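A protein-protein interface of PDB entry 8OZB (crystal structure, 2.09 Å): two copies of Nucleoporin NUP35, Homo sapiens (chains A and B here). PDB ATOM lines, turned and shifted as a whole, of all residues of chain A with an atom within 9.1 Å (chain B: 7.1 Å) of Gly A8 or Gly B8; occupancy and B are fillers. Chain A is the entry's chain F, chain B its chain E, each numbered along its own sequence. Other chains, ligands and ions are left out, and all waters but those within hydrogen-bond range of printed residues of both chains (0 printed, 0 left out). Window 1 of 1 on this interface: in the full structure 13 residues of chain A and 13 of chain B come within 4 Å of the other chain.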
ATOM      1  N   THR A   5       2.802   9.958   8.330  1.00  0.00           N
ATOM      2  CA  THR A   5       3.950  10.201   9.226  1.00  0.00           C
ATOM      3  C   THR A   5       5.219   9.953   8.407  1.00  0.00           C
ATOM      4  O   THR A   5       5.406   8.825   7.876  1.00  0.00           O
ATOM      5  CB  THR A   5       3.788   9.380  10.509  1.00  0.00           C
ATOM      6  OG1 THR A   5       2.532   9.826  11.021  1.00  0.00           O
ATOM      7  CG2 THR A   5       4.926   9.575  11.491  1.00  0.00           C
ATOM      8  N   VAL A   6       6.006  11.016   8.264  1.00  0.00           N
ATOM      9  CA  VAL A   6       7.345  11.008   7.642  1.00  0.00           C
ATOM     10  C   VAL A   6       8.363  10.948   8.784  1.00  0.00           C
ATOM     11  O   VAL A   6       8.229  11.702   9.755  1.00  0.00           O
ATOM     12  CB  VAL A   6       7.526  12.282   6.808  1.00  0.00           C
ATOM     13  CG1 VAL A   6       8.903  12.322   6.157  1.00  0.00           C
ATOM     14  CG2 VAL A   6       6.404  12.424   5.789  1.00  0.00           C
ATOM     15  N   PHE A   7       9.365  10.095   8.692  1.00  0.00           N
ATOM     16  CA  PHE A   7      10.296   9.905   9.827  1.00  0.00           C
ATOM     17  C   PHE A   7      11.677   9.543   9.300  1.00  0.00           C
ATOM     18  O   PHE A   7      11.868   9.068   8.130  1.00  0.00           O
ATOM     19  CB  PHE A   7       9.721   8.875  10.810  1.00  0.00           C
ATOM     20  CG  PHE A   7       9.606   7.461  10.286  1.00  0.00           C
ATOM     21  CD1 PHE A   7      10.671   6.573  10.402  1.00  0.00           C
ATOM     22  CD2 PHE A   7       8.444   7.022   9.657  1.00  0.00           C
ATOM     23  CE1 PHE A   7      10.557   5.280   9.911  1.00  0.00           C
ATOM     24  CE2 PHE A   7       8.316   5.712   9.213  1.00  0.00           C
ATOM     25  CZ  PHE A   7       9.379   4.849   9.329  1.00  0.00           C
ATOM     26  N   GLY A   8      12.621   9.716  10.213  1.00  0.00           N
ATOM     27  CA  GLY A   8      13.976   9.168  10.087  1.00  0.00           C
ATOM     28  C   GLY A   8      15.006  10.247   9.857  1.00  0.00           C
ATOM     29  O   GLY A   8      16.133   9.893   9.527  1.00  0.00           O
ATOM     30  N   PHE A   9      14.632  11.515   9.989  1.00  0.00           N
ATOM     31  CA  PHE A   9      15.506  12.661   9.629  1.00  0.00           C
ATOM     32  C   PHE A   9      15.969  13.323  10.913  1.00  0.00           C
ATOM     33  O   PHE A   9      15.216  13.368  11.848  1.00  0.00           O
ATOM     34  CB  PHE A   9      14.746  13.658   8.744  1.00  0.00           C
ATOM     35  CG  PHE A   9      13.421  14.062   9.331  1.00  0.00           C
ATOM     36  CD1 PHE A   9      13.343  15.081  10.261  1.00  0.00           C
ATOM     37  CD2 PHE A   9      12.273  13.355   9.021  1.00  0.00           C
ATOM     38  CE1 PHE A   9      12.140  15.381  10.873  1.00  0.00           C
ATOM     39  CE2 PHE A   9      11.072  13.670   9.623  1.00  0.00           C
ATOM     40  CZ  PHE A   9      11.001  14.698  10.529  1.00  0.00           C
ATOM     41  N   PRO A  10      17.163  13.927  10.965  1.00  0.00           N
ATOM     42  CA  PRO A  10      17.550  14.797  12.085  1.00  0.00           C
ATOM     43  C   PRO A  10      16.839  16.173  12.118  1.00  0.00           C
ATOM     44  O   PRO A  10      16.329  16.668  11.089  1.00  0.00           O
ATOM     45  CB  PRO A  10      19.068  14.987  11.890  1.00  0.00           C
ATOM     46  CG  PRO A  10      19.357  14.651  10.421  1.00  0.00           C
ATOM     47  CD  PRO A  10      18.197  13.806   9.919  1.00  0.00           C
ATOM     48  N   GLN A  11      16.751  16.781  13.303  1.00  0.00           N
ATOM     49  CA  GLN A  11      15.988  18.049  13.515  1.00  0.00           C
ATOM     50  C   GLN A  11      16.474  19.094  12.505  1.00  0.00           C
ATOM     51  O   GLN A  11      15.600  19.800  11.953  1.00  0.00           O
ATOM     52  CB  GLN A  11      16.114  18.586  14.941  1.00  0.00           C
ATOM     53  CG  GLN A  11      15.523  17.651  15.994  1.00  0.00           C
ATOM     54  CD  GLN A  11      14.077  17.884  16.381  1.00  0.00           C
ATOM     55  OE1 GLN A  11      13.158  17.904  15.554  1.00  0.00           O
ATOM     56  NE2 GLN A  11      13.856  17.996  17.684  1.00  0.00           N
ATOM     57  N   SER A  13      17.248  18.910   9.509  1.00  0.00           N
ATOM     58  CA  SER A  13      16.855  18.600   8.109  1.00  0.00           C
ATOM     59  C   SER A  13      15.349  18.692   7.943  1.00  0.00           C
ATOM     60  O   SER A  13      14.885  18.383   6.852  1.00  0.00           O
ATOM     61  CB  SER A  13      17.297  17.213   7.697  1.00  0.00           C
ATOM     62  OG  SER A  13      18.692  17.157   7.497  1.00  0.00           O
ATOM     63  N   ALA A  14      14.619  18.991   9.004  1.00  0.00           N
ATOM     64  CA  ALA A  14      13.150  18.831   9.034  1.00  0.00           C
ATOM     65  C   ALA A  14      12.553  19.648   7.906  1.00  0.00           C
ATOM     66  O   ALA A  14      11.661  19.170   7.171  1.00  0.00           O
ATOM     67  CB  ALA A  14      12.589  19.264  10.359  1.00  0.00           C
ATOM     68  N   ILE A  17      13.160  18.336   4.472  1.00  0.00           N
ATOM     69  CA  ILE A  17      12.332  17.112   4.183  1.00  0.00           C
ATOM     70  C   ILE A  17      10.889  17.536   3.897  1.00  0.00           C
ATOM     71  O   ILE A  17      10.280  16.987   2.955  1.00  0.00           O
ATOM     72  CB  ILE A  17      12.471  16.058   5.305  1.00  0.00           C
ATOM     73  CG1 ILE A  17      13.901  15.491   5.358  1.00  0.00           C
ATOM     74  CG2 ILE A  17      11.435  14.971   5.168  1.00  0.00           C
ATOM     75  CD1 ILE A  17      14.431  14.882   4.077  1.00  0.00           C
ATOM     76  N   PHE A  21       8.533  16.843   0.670  1.00  0.00           N
ATOM     77  CA  PHE A  21       7.182  16.208   0.720  1.00  0.00           C
ATOM     78  C   PHE A  21       6.078  17.138   0.193  1.00  0.00           C
ATOM     79  O   PHE A  21       5.013  16.608  -0.224  1.00  0.00           O
ATOM     80  CB  PHE A  21       6.880  15.622   2.097  1.00  0.00           C
ATOM     81  CG  PHE A  21       7.458  14.240   2.185  1.00  0.00           C
ATOM     82  CD1 PHE A  21       6.695  13.140   1.843  1.00  0.00           C
ATOM     83  CD2 PHE A  21       8.795  14.058   2.480  1.00  0.00           C
ATOM     84  CE1 PHE A  21       7.253  11.872   1.847  1.00  0.00           C
ATOM     85  CE2 PHE A  21       9.357  12.793   2.466  1.00  0.00           C
ATOM     86  CZ  PHE A  21       8.581  11.703   2.161  1.00  0.00           C
ATOM     87  N   GLY A  36      11.227  13.707  18.784  1.00  0.00           N
ATOM     88  CA  GLY A  36      11.264  12.570  17.847  1.00  0.00           C
ATOM     89  C   GLY A  36      11.862  12.936  16.503  1.00  0.00           C
ATOM     90  O   GLY A  36      12.060  14.099  16.218  1.00  0.00           O
ATOM     91  N   ASN A  37      12.112  11.952  15.664  1.00  0.00           N
ATOM     92  CA  ASN A  37      12.673  12.184  14.317  1.00  0.00           C
ATOM     93  C   ASN A  37      11.523  12.057  13.315  1.00  0.00           C
ATOM     94  O   ASN A  37      11.683  11.362  12.319  1.00  0.00           O
ATOM     95  CB  ASN A  37      13.809  11.205  14.089  1.00  0.00           C
ATOM     96  CG  ASN A  37      13.315   9.775  14.147  1.00  0.00           C
ATOM     97  OD1 ASN A  37      12.292   9.475  14.788  1.00  0.00           O
ATOM     98  ND2 ASN A  37      14.010   8.907  13.436  1.00  0.00           N
ATOM     99  N   TRP A  38      10.371  12.643  13.597  1.00  0.00           N
ATOM    100  CA  TRP A  38       9.178  12.440  12.745  1.00  0.00           C
ATOM    101  C   TRP A  38       8.309  13.690  12.711  1.00  0.00           C
ATOM    102  O   TRP A  38       8.396  14.519  13.629  1.00  0.00           O
ATOM    103  CB  TRP A  38       8.385  11.195  13.184  1.00  0.00           C
ATOM    104  CG  TRP A  38       7.721  11.298  14.522  1.00  0.00           C
ATOM    105  CD1 TRP A  38       6.527  11.898  14.808  1.00  0.00           C
ATOM    106  CD2 TRP A  38       8.206  10.752  15.757  1.00  0.00           C
ATOM    107  NE1 TRP A  38       6.261  11.800  16.141  1.00  0.00           N
ATOM    108  CE2 TRP A  38       7.269  11.101  16.753  1.00  0.00           C
ATOM    109  CE3 TRP A  38       9.347  10.037  16.129  1.00  0.00           C
ATOM    110  CZ2 TRP A  38       7.439  10.737  18.092  1.00  0.00           C
ATOM    111  CZ3 TRP A  38       9.512   9.665  17.451  1.00  0.00           C
ATOM    112  CH2 TRP A  38       8.573  10.022  18.422  1.00  0.00           C
ATOM    113  N   MET A  39       7.450  13.754  11.695  1.00  0.00           N
ATOM    114  CA  MET A  39       6.394  14.778  11.526  1.00  0.00           C
ATOM    115  C   MET A  39       5.178  14.122  10.864  1.00  0.00           C
ATOM    116  O   MET A  39       5.338  13.059  10.184  1.00  0.00           O
ATOM    117  CB  MET A  39       6.904  15.944  10.683  1.00  0.00           C
ATOM    118  CG  MET A  39       7.253  15.532   9.280  1.00  0.00           C
ATOM    119  SD  MET A  39       7.869  16.875   8.213  1.00  0.00           S
ATOM    120  CE  MET A  39       9.348  17.407   9.053  1.00  0.00           C
ATOM    121  N   ASP A  56       8.523   5.778   0.928  1.00  0.00           N
ATOM    122  CA  ASP A  56       9.002   4.973   2.066  1.00  0.00           C
ATOM    123  C   ASP A  56      10.259   4.222   1.626  1.00  0.00           C
ATOM    124  O   ASP A  56      10.182   3.466   0.663  1.00  0.00           O
ATOM    125  CB  ASP A  56       7.888   4.040   2.523  1.00  0.00           C
ATOM    126  CG  ASP A  56       8.156   3.317   3.830  1.00  0.00           C
ATOM    127  OD1 ASP A  56       8.700   3.951   4.774  1.00  0.00           O
ATOM    128  OD2 ASP A  56       7.793   2.131   3.898  1.00  0.00           O
ATOM    129  N   GLY A  57      11.390   4.488   2.279  1.00  0.00           N
ATOM    130  CA  GLY A  57      12.648   3.744   2.087  1.00  0.00           C
ATOM    131  C   GLY A  57      13.563   4.436   1.110  1.00  0.00           C
ATOM    132  O   GLY A  57      14.658   3.904   0.881  1.00  0.00           O
ATOM    133  N   ARG A  58      13.128   5.565   0.540  1.00  0.00           N
ATOM    134  CA  ARG A  58      13.903   6.327  -0.474  1.00  0.00           C
ATOM    135  C   ARG A  58      14.865   7.289   0.238  1.00  0.00           C
ATOM    136  O   ARG A  58      14.602   7.726   1.376  1.00  0.00           O
ATOM    137  CB  ARG A  58      12.982   7.086  -1.441  1.00  0.00           C
ATOM    138  CG  ARG A  58      12.006   6.216  -2.229  1.00  0.00           C
ATOM    139  CD  ARG A  58      12.672   5.259  -3.197  1.00  0.00           C
ATOM    140  NE  ARG A  58      13.631   5.986  -4.023  1.00  0.00           N
ATOM    141  CZ  ARG A  58      13.316   6.776  -5.057  1.00  0.00           C
ATOM    142  NH1 ARG A  58      12.054   6.932  -5.432  1.00  0.00           N
ATOM    143  NH2 ARG A  58      14.274   7.405  -5.721  1.00  0.00           N
ATOM    144  N   PHE A  60      16.814  10.886   0.467  1.00  0.00           N
ATOM    145  CA  PHE A  60      16.656  12.320   0.151  1.00  0.00           C
ATOM    146  C   PHE A  60      17.959  12.997   0.546  1.00  0.00           C
ATOM    147  O   PHE A  60      18.590  12.518   1.517  1.00  0.00           O
ATOM    148  CB  PHE A  60      15.450  12.890   0.904  1.00  0.00           C
ATOM    149  CG  PHE A  60      14.120  12.375   0.422  1.00  0.00           C
ATOM    150  CD1 PHE A  60      13.312  13.146  -0.400  1.00  0.00           C
ATOM    151  CD2 PHE A  60      13.683  11.111   0.772  1.00  0.00           C
ATOM    152  CE1 PHE A  60      12.072  12.687  -0.810  1.00  0.00           C
ATOM    153  CE2 PHE A  60      12.446  10.647   0.353  1.00  0.00           C
ATOM    154  CZ  PHE A  60      11.647  11.429  -0.450  1.00  0.00           C
ATOM    155  N   SER A  63      21.876  11.591   1.582  1.00  0.00           N
ATOM    156  CA  SER A  63      22.268  10.821   2.793  1.00  0.00           C
ATOM    157  C   SER A  63      21.127  10.606   3.792  1.00  0.00           C
ATOM    158  O   SER A  63      21.443  10.130   4.897  1.00  0.00           O
ATOM    159  CB  SER A  63      23.416  11.498   3.488  1.00  0.00           C
ATOM    160  OG  SER A  63      23.016  12.789   3.900  1.00  0.00           O
ATOM    161  N   ILE A  64      19.871  10.933   3.484  1.00  0.00           N
ATOM    162  CA  ILE A  64      18.779  10.731   4.488  1.00  0.00           C
ATOM    163  C   ILE A  64      17.762   9.770   3.894  1.00  0.00           C
ATOM    164  O   ILE A  64      16.993  10.186   2.999  1.00  0.00           O
ATOM    165  CB  ILE A  64      18.114  12.040   4.953  1.00  0.00           C
ATOM    166  CG1 ILE A  64      19.139  13.124   5.331  1.00  0.00           C
ATOM    167  CG2 ILE A  64      17.143  11.741   6.087  1.00  0.00           C
ATOM    168  CD1 ILE A  64      18.515  14.481   5.691  1.00  0.00           C
ATOM    169  N   MET A  65      17.813   8.519   4.339  1.00  0.00           N
ATOM    170  CA  MET A  65      16.788   7.516   4.006  1.00  0.00           C
ATOM    171  C   MET A  65      15.577   7.839   4.890  1.00  0.00           C
ATOM    172  O   MET A  65      15.764   8.109   6.085  1.00  0.00           O
ATOM    173  CB  MET A  65      17.299   6.103   4.293  1.00  0.00           C
ATOM    174  CG  MET A  65      16.377   5.040   3.766  1.00  0.00           C
ATOM    175  SD  MET A  65      17.146   3.427   3.834  1.00  0.00           S
ATOM    176  CE  MET A  65      18.501   3.606   2.673  1.00  0.00           C
ATOM    177  N   ILE A  66      14.385   7.837   4.306  1.00  0.00           N
ATOM    178  CA  ILE A  66      13.142   8.400   4.886  1.00  0.00           C
ATOM    179  C   ILE A  66      12.108   7.294   4.926  1.00  0.00           C
ATOM    180  O   ILE A  66      11.949   6.577   3.914  1.00  0.00           O
ATOM    181  CB  ILE A  66      12.645   9.582   4.041  1.00  0.00           C
ATOM    182  CG1 ILE A  66      13.547  10.798   4.188  1.00  0.00           C
ATOM    183  CG2 ILE A  66      11.205   9.910   4.387  1.00  0.00           C
ATOM    184  CD1 ILE A  66      13.553  11.353   5.579  1.00  0.00           C
ATOM    185  N   GLY A  67      11.428   7.197   6.061  1.00  0.00           N
ATOM    186  CA  GLY A  67      10.255   6.340   6.262  1.00  0.00           C
ATOM    187  C   GLY A  67       8.995   7.159   6.152  1.00  0.00           C
ATOM    188  O   GLY A  67       9.000   8.335   6.551  1.00  0.00           O
ATOM    189  N   VAL A  68       7.949   6.569   5.595  1.00  0.00           N
ATOM    190  CA  VAL A  68       6.603   7.196   5.457  1.00  0.00           C
ATOM    191  C   VAL A  68       5.588   6.086   5.752  1.00  0.00           C
ATOM    192  O   VAL A  68       5.660   5.050   5.106  1.00  0.00           O
ATOM    193  CB  VAL A  68       6.375   7.784   4.044  1.00  0.00           C
ATOM    194  CG1 VAL A  68       5.114   8.633   4.008  1.00  0.00           C
ATOM    195  CG2 VAL A  68       7.573   8.554   3.482  1.00  0.00           C
ATOM    196  N   VAL B   6      18.279  -1.166   8.123  1.00  0.00           N
ATOM    197  CA  VAL B   6      17.667  -0.410   9.240  1.00  0.00           C
ATOM    198  C   VAL B   6      18.037   1.068   9.054  1.00  0.00           C
ATOM    199  O   VAL B   6      19.200   1.376   8.763  1.00  0.00           O
ATOM    200  CB  VAL B   6      18.157  -0.974  10.574  1.00  0.00           C
ATOM    201  CG1 VAL B   6      17.687  -0.125  11.738  1.00  0.00           C
ATOM    202  CG2 VAL B   6      17.723  -2.429  10.722  1.00  0.00           C
ATOM    203  N   PHE B   7      17.085   1.968   9.187  1.00  0.00           N
ATOM    204  CA  PHE B   7      17.353   3.377   8.842  1.00  0.00           C
ATOM    205  C   PHE B   7      16.522   4.292   9.745  1.00  0.00           C
ATOM    206  O   PHE B   7      15.498   3.850  10.354  1.00  0.00           O
ATOM    207  CB  PHE B   7      17.116   3.582   7.342  1.00  0.00           C
ATOM    208  CG  PHE B   7      15.673   3.494   6.906  1.00  0.00           C
ATOM    209  CD1 PHE B   7      14.844   4.611   6.954  1.00  0.00           C
ATOM    210  CD2 PHE B   7      15.142   2.300   6.433  1.00  0.00           C
ATOM    211  CE1 PHE B   7      13.527   4.530   6.527  1.00  0.00           C
ATOM    212  CE2 PHE B   7      13.826   2.218   6.017  1.00  0.00           C
ATOM    213  CZ  PHE B   7      13.025   3.340   6.045  1.00  0.00           C
ATOM    214  N   GLY B   8      16.982   5.541   9.795  1.00  0.00           N
ATOM    215  CA  GLY B   8      16.207   6.698  10.267  1.00  0.00           C
ATOM    216  C   GLY B   8      16.777   7.251  11.543  1.00  0.00           C
ATOM    217  O   GLY B   8      16.071   7.996  12.164  1.00  0.00           O
ATOM    218  N   PHE B   9      18.003   6.873  11.914  1.00  0.00           N
ATOM    219  CA  PHE B   9      18.608   7.164  13.240  1.00  0.00           C
ATOM    220  C   PHE B   9      19.801   8.063  13.002  1.00  0.00           C
ATOM    221  O   PHE B   9      20.443   7.975  11.967  1.00  0.00           O
ATOM    222  CB  PHE B   9      19.105   5.899  13.976  1.00  0.00           C
ATOM    223  CG  PHE B   9      20.037   5.047  13.156  1.00  0.00           C
ATOM    224  CD1 PHE B   9      21.381   5.360  13.056  1.00  0.00           C
ATOM    225  CD2 PHE B   9      19.528   4.001  12.387  1.00  0.00           C
ATOM    226  CE1 PHE B   9      22.206   4.620  12.228  1.00  0.00           C
ATOM    227  CE2 PHE B   9      20.346   3.264  11.561  1.00  0.00           C
ATOM    228  CZ  PHE B   9      21.691   3.555  11.505  1.00  0.00           C
ATOM    229  N   PRO B  10      20.118   8.908  13.983  1.00  0.00           N
ATOM    230  CA  PRO B  10      21.339   9.708  13.956  1.00  0.00           C
ATOM    231  C   PRO B  10      22.596   8.878  14.299  1.00  0.00           C
ATOM    232  O   PRO B  10      22.494   7.909  15.014  1.00  0.00           O
ATOM    233  CB  PRO B  10      21.049  10.804  15.000  1.00  0.00           C
ATOM    234  CG  PRO B  10      19.990  10.239  15.934  1.00  0.00           C
ATOM    235  CD  PRO B  10      19.252   9.166  15.150  1.00  0.00           C
ATOM    236  N   ASN B  37      21.908   7.646   7.192  1.00  0.00           N
ATOM    237  CA  ASN B  37      21.251   7.357   8.481  1.00  0.00           C
ATOM    238  C   ASN B  37      20.789   5.887   8.472  1.00  0.00           C
ATOM    239  O   ASN B  37      19.647   5.616   8.908  1.00  0.00           O
ATOM    240  CB  ASN B  37      20.101   8.331   8.723  1.00  0.00           C
ATOM    241  CG  ASN B  37      19.032   8.235   7.659  1.00  0.00           C
ATOM    242  OD1 ASN B  37      19.316   7.824   6.524  1.00  0.00           O
ATOM    243  ND2 ASN B  37      17.814   8.621   8.002  1.00  0.00           N
ATOM    244  N   TRP B  38      21.594   4.970   7.936  1.00  0.00           N
ATOM    245  CA  TRP B  38      21.171   3.559   7.743  1.00  0.00           C
ATOM    246  C   TRP B  38      22.313   2.569   8.003  1.00  0.00           C
ATOM    247  O   TRP B  38      23.471   2.960   7.961  1.00  0.00           O
ATOM    248  CB  TRP B  38      20.548   3.376   6.359  1.00  0.00           C
ATOM    249  CG  TRP B  38      21.462   3.549   5.191  1.00  0.00           C
ATOM    250  CD1 TRP B  38      22.308   2.615   4.670  1.00  0.00           C
ATOM    251  CD2 TRP B  38      21.578   4.711   4.348  1.00  0.00           C
ATOM    252  NE1 TRP B  38      22.991   3.136   3.608  1.00  0.00           N
ATOM    253  CE2 TRP B  38      22.555   4.418   3.378  1.00  0.00           C
ATOM    254  CE3 TRP B  38      20.965   5.964   4.326  1.00  0.00           C
ATOM    255  CZ2 TRP B  38      22.895   5.321   2.369  1.00  0.00           C
ATOM    256  CZ3 TRP B  38      21.321   6.872   3.348  1.00  0.00           C
ATOM    257  CH2 TRP B  38      22.282   6.556   2.384  1.00  0.00           C
ATOM    258  N   MET B  39      21.969   1.294   8.159  1.00  0.00           N
ATOM    259  CA  MET B  39      22.942   0.168   8.264  1.00  0.00           C
ATOM    260  C   MET B  39      22.287  -1.096   7.675  1.00  0.00           C
ATOM    261  O   MET B  39      21.029  -1.235   7.708  1.00  0.00           O
ATOM    262  CB  MET B  39      23.421  -0.067   9.713  1.00  0.00           C
ATOM    263  CG  MET B  39      22.315  -0.521  10.630  1.00  0.00           C
ATOM    264  SD  MET B  39      22.692  -0.833  12.405  1.00  0.00           S
ATOM    265  CE  MET B  39      23.259   0.789  12.885  1.00  0.00           C
ATOM    266  N   SER B  63      12.277   8.220  21.285  1.00  0.00           N
ATOM    267  CA  SER B  63      12.283   9.366  20.338  1.00  0.00           C
ATOM    268  C   SER B  63      12.867   8.996  18.964  1.00  0.00           C
ATOM    269  O   SER B  63      12.991   9.899  18.130  1.00  0.00           O
ATOM    270  CB  SER B  63      13.048  10.492  20.956  1.00  0.00           C
ATOM    271  OG  SER B  63      14.352  10.036  21.260  1.00  0.00           O
ATOM    272  N   ILE B  64      13.247   7.739  18.724  1.00  0.00           N
ATOM    273  CA  ILE B  64      13.811   7.339  17.404  1.00  0.00           C
ATOM    274  C   ILE B  64      12.865   6.327  16.769  1.00  0.00           C
ATOM    275  O   ILE B  64      12.893   5.153  17.162  1.00  0.00           O
ATOM    276  CB  ILE B  64      15.248   6.795  17.475  1.00  0.00           C
ATOM    277  CG1 ILE B  64      16.140   7.651  18.388  1.00  0.00           C
ATOM    278  CG2 ILE B  64      15.797   6.691  16.060  1.00  0.00           C
ATOM    279  CD1 ILE B  64      17.605   7.225  18.420  1.00  0.00           C
ATOM    280  N   MET B  65      12.087   6.824  15.810  1.00  0.00           N
ATOM    281  CA  MET B  65      11.284   6.037  14.881  1.00  0.00           C
ATOM    282  C   MET B  65      12.228   5.503  13.813  1.00  0.00           C
ATOM    283  O   MET B  65      13.118   6.255  13.351  1.00  0.00           O
ATOM    284  CB  MET B  65      10.190   6.906  14.269  1.00  0.00           C
ATOM    285  CG  MET B  65       9.118   6.096  13.593  1.00  0.00           C
ATOM    286  SD  MET B  65       7.640   7.092  13.205  1.00  0.00           S
ATOM    287  CE  MET B  65       7.030   6.053  11.899  1.00  0.00           C
ATOM    288  N   ILE B  66      12.049   4.223  13.498  1.00  0.00           N
ATOM    289  CA  ILE B  66      13.009   3.353  12.765  1.00  0.00           C
ATOM    290  C   ILE B  66      12.305   2.710  11.572  1.00  0.00           C
ATOM    291  O   ILE B  66      11.177   2.158  11.723  1.00  0.00           O
ATOM    292  CB  ILE B  66      13.591   2.278  13.699  1.00  0.00           C
ATOM    293  CG1 ILE B  66      14.489   2.899  14.772  1.00  0.00           C
ATOM    294  CG2 ILE B  66      14.300   1.206  12.875  1.00  0.00           C
ATOM    295  CD1 ILE B  66      15.793   3.424  14.269  1.00  0.00           C
ATOM    296  N   GLY B  67      12.981   2.797  10.438  1.00  0.00           N
ATOM    297  CA  GLY B  67      12.605   2.125   9.189  1.00  0.00           C
ATOM    298  C   GLY B  67      13.419   0.873   9.027  1.00  0.00           C
ATOM    299  O   GLY B  67      14.575   0.843   9.467  1.00  0.00           O
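Thr A5 touches none of the printed residues of chain B.
Of chain B, only Gly B8 (3.2 Å) and Asn B37 (2.6 Å) come within 4 Å of Gly A8.
Printed residues of chain B within 4 Å of Gly A36: Ser B63.
Of the printed residues of chain B, Asn A37 touches Gly B8 (2.6 Å), Ser B63 (3.3 Å), Ile B64 (3.7 Å) and Met B65 (2.8 Å).
Printed residues of chain B within 4 Å of Ile A64: Asn B37 (3.6 Å).
Of chain A, only Gly A8 (3.2 Å) and Asn A37 (2.6 Å) come within 4 Å of Gly B8.
Pro B10 touches none of the printed residues of chain A.
The nearest residue of chain B that does not touch Gly A8 is Phe B9 (4.3 Å).
The nearest residue of chain A that does not touch Gly B8 is Phe A9 (4.4 Å).
Met B65 touches Phe A7 (CE to CD2, 2.8 Å).
Phe A7 touches Ile B66.
CE1 of Phe A7 touches N of Gly B67, at 3.5 Å.
Asn A37 touches Ile B64.
CB of Met B65 touches CE3 of Trp A38 (3.7 Å).
CA of Ile A64 touches OD1 of Asn B37, 3.6 Å away.
Met A65 touches Phe B7.
CB of Met A65 touches CE3 of Trp B38, 3.7 Å away.
Ile A66 touches Phe B7.
Gly A67 touches Phe B7 (N to CE1, 3.4 Å).
Of the 13 printed residues of chain B, 9 touch a printed residue of chain A.
Printed residues of chain B that touch a printed residue of chain A: Phe B7, Gly B8, Asn B37, Trp B38, Ser B63, Ile B64, Met B65, Ile B66 and Gly B67.
Hydrophobic or aromatic side chains of chain B that line the printed part of chain A: Phe B7, Trp B38, Ile B64 and Met B65.
Among the printed residues, 21 pairs touch across the chains.
Phe A7 touches Met B65, and with the chains exchanged Met A65 touches Phe B7.
Phe A7 touches Gly B67, and with the chains exchanged Gly A67 touches Phe B7.
Asn A37 touches Ser B63, and with the chains exchanged Ser A63 touches Asn B37.
Trp A38 touches Met B65, and with the chains exchanged Met A65 touches Trp B38.
O of Gly B8 is in hydrogen-bond range of ND2 of Asn A37 (2.6 Å).
ND2 of Asn B37 is in hydrogen-bond range of O of Gly A8 (2.6 Å).
The backbone carbonyl oxygen of Ser A63 lies within hydrogen-bond range of the backbone NH of Asn B37, at 3.4 Å.
The backbone NH (N) of Met A65 is in hydrogen-bond range of the side-chain amide oxygen (OD1) of Asn B37 (2.7 Å).
N of Asn A37 lies within hydrogen-bond range of O of Ser B63, at 3.3 Å.
O of Met B65 lies within hydrogen-bond range of ND2 of Asn A37 (2.8 Å).
O of Gly A8 sits close to O of Gly B8 (3.2 Å).
The backbone carbonyl oxygen of Phe B7 sits at hydrogen-bond distance from the backbone NH of Gly B67.
N of Gly B8 is in hydrogen-bond range of O of Asn B37 (2.8 Å).
The backbone carbonyl oxygen (O) of Gly A67 sits at hydrogen-bond distance from the backbone NH (N) of Phe A7, 2.8 Å away.
O of Asn A37 is in hydrogen-bond range of N of Gly A8 (2.8 Å).
N of Gly A57 lies within hydrogen-bond range of O of Ile A66.
O of Arg A58 sits at hydrogen-bond distance from N of Ile A66.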
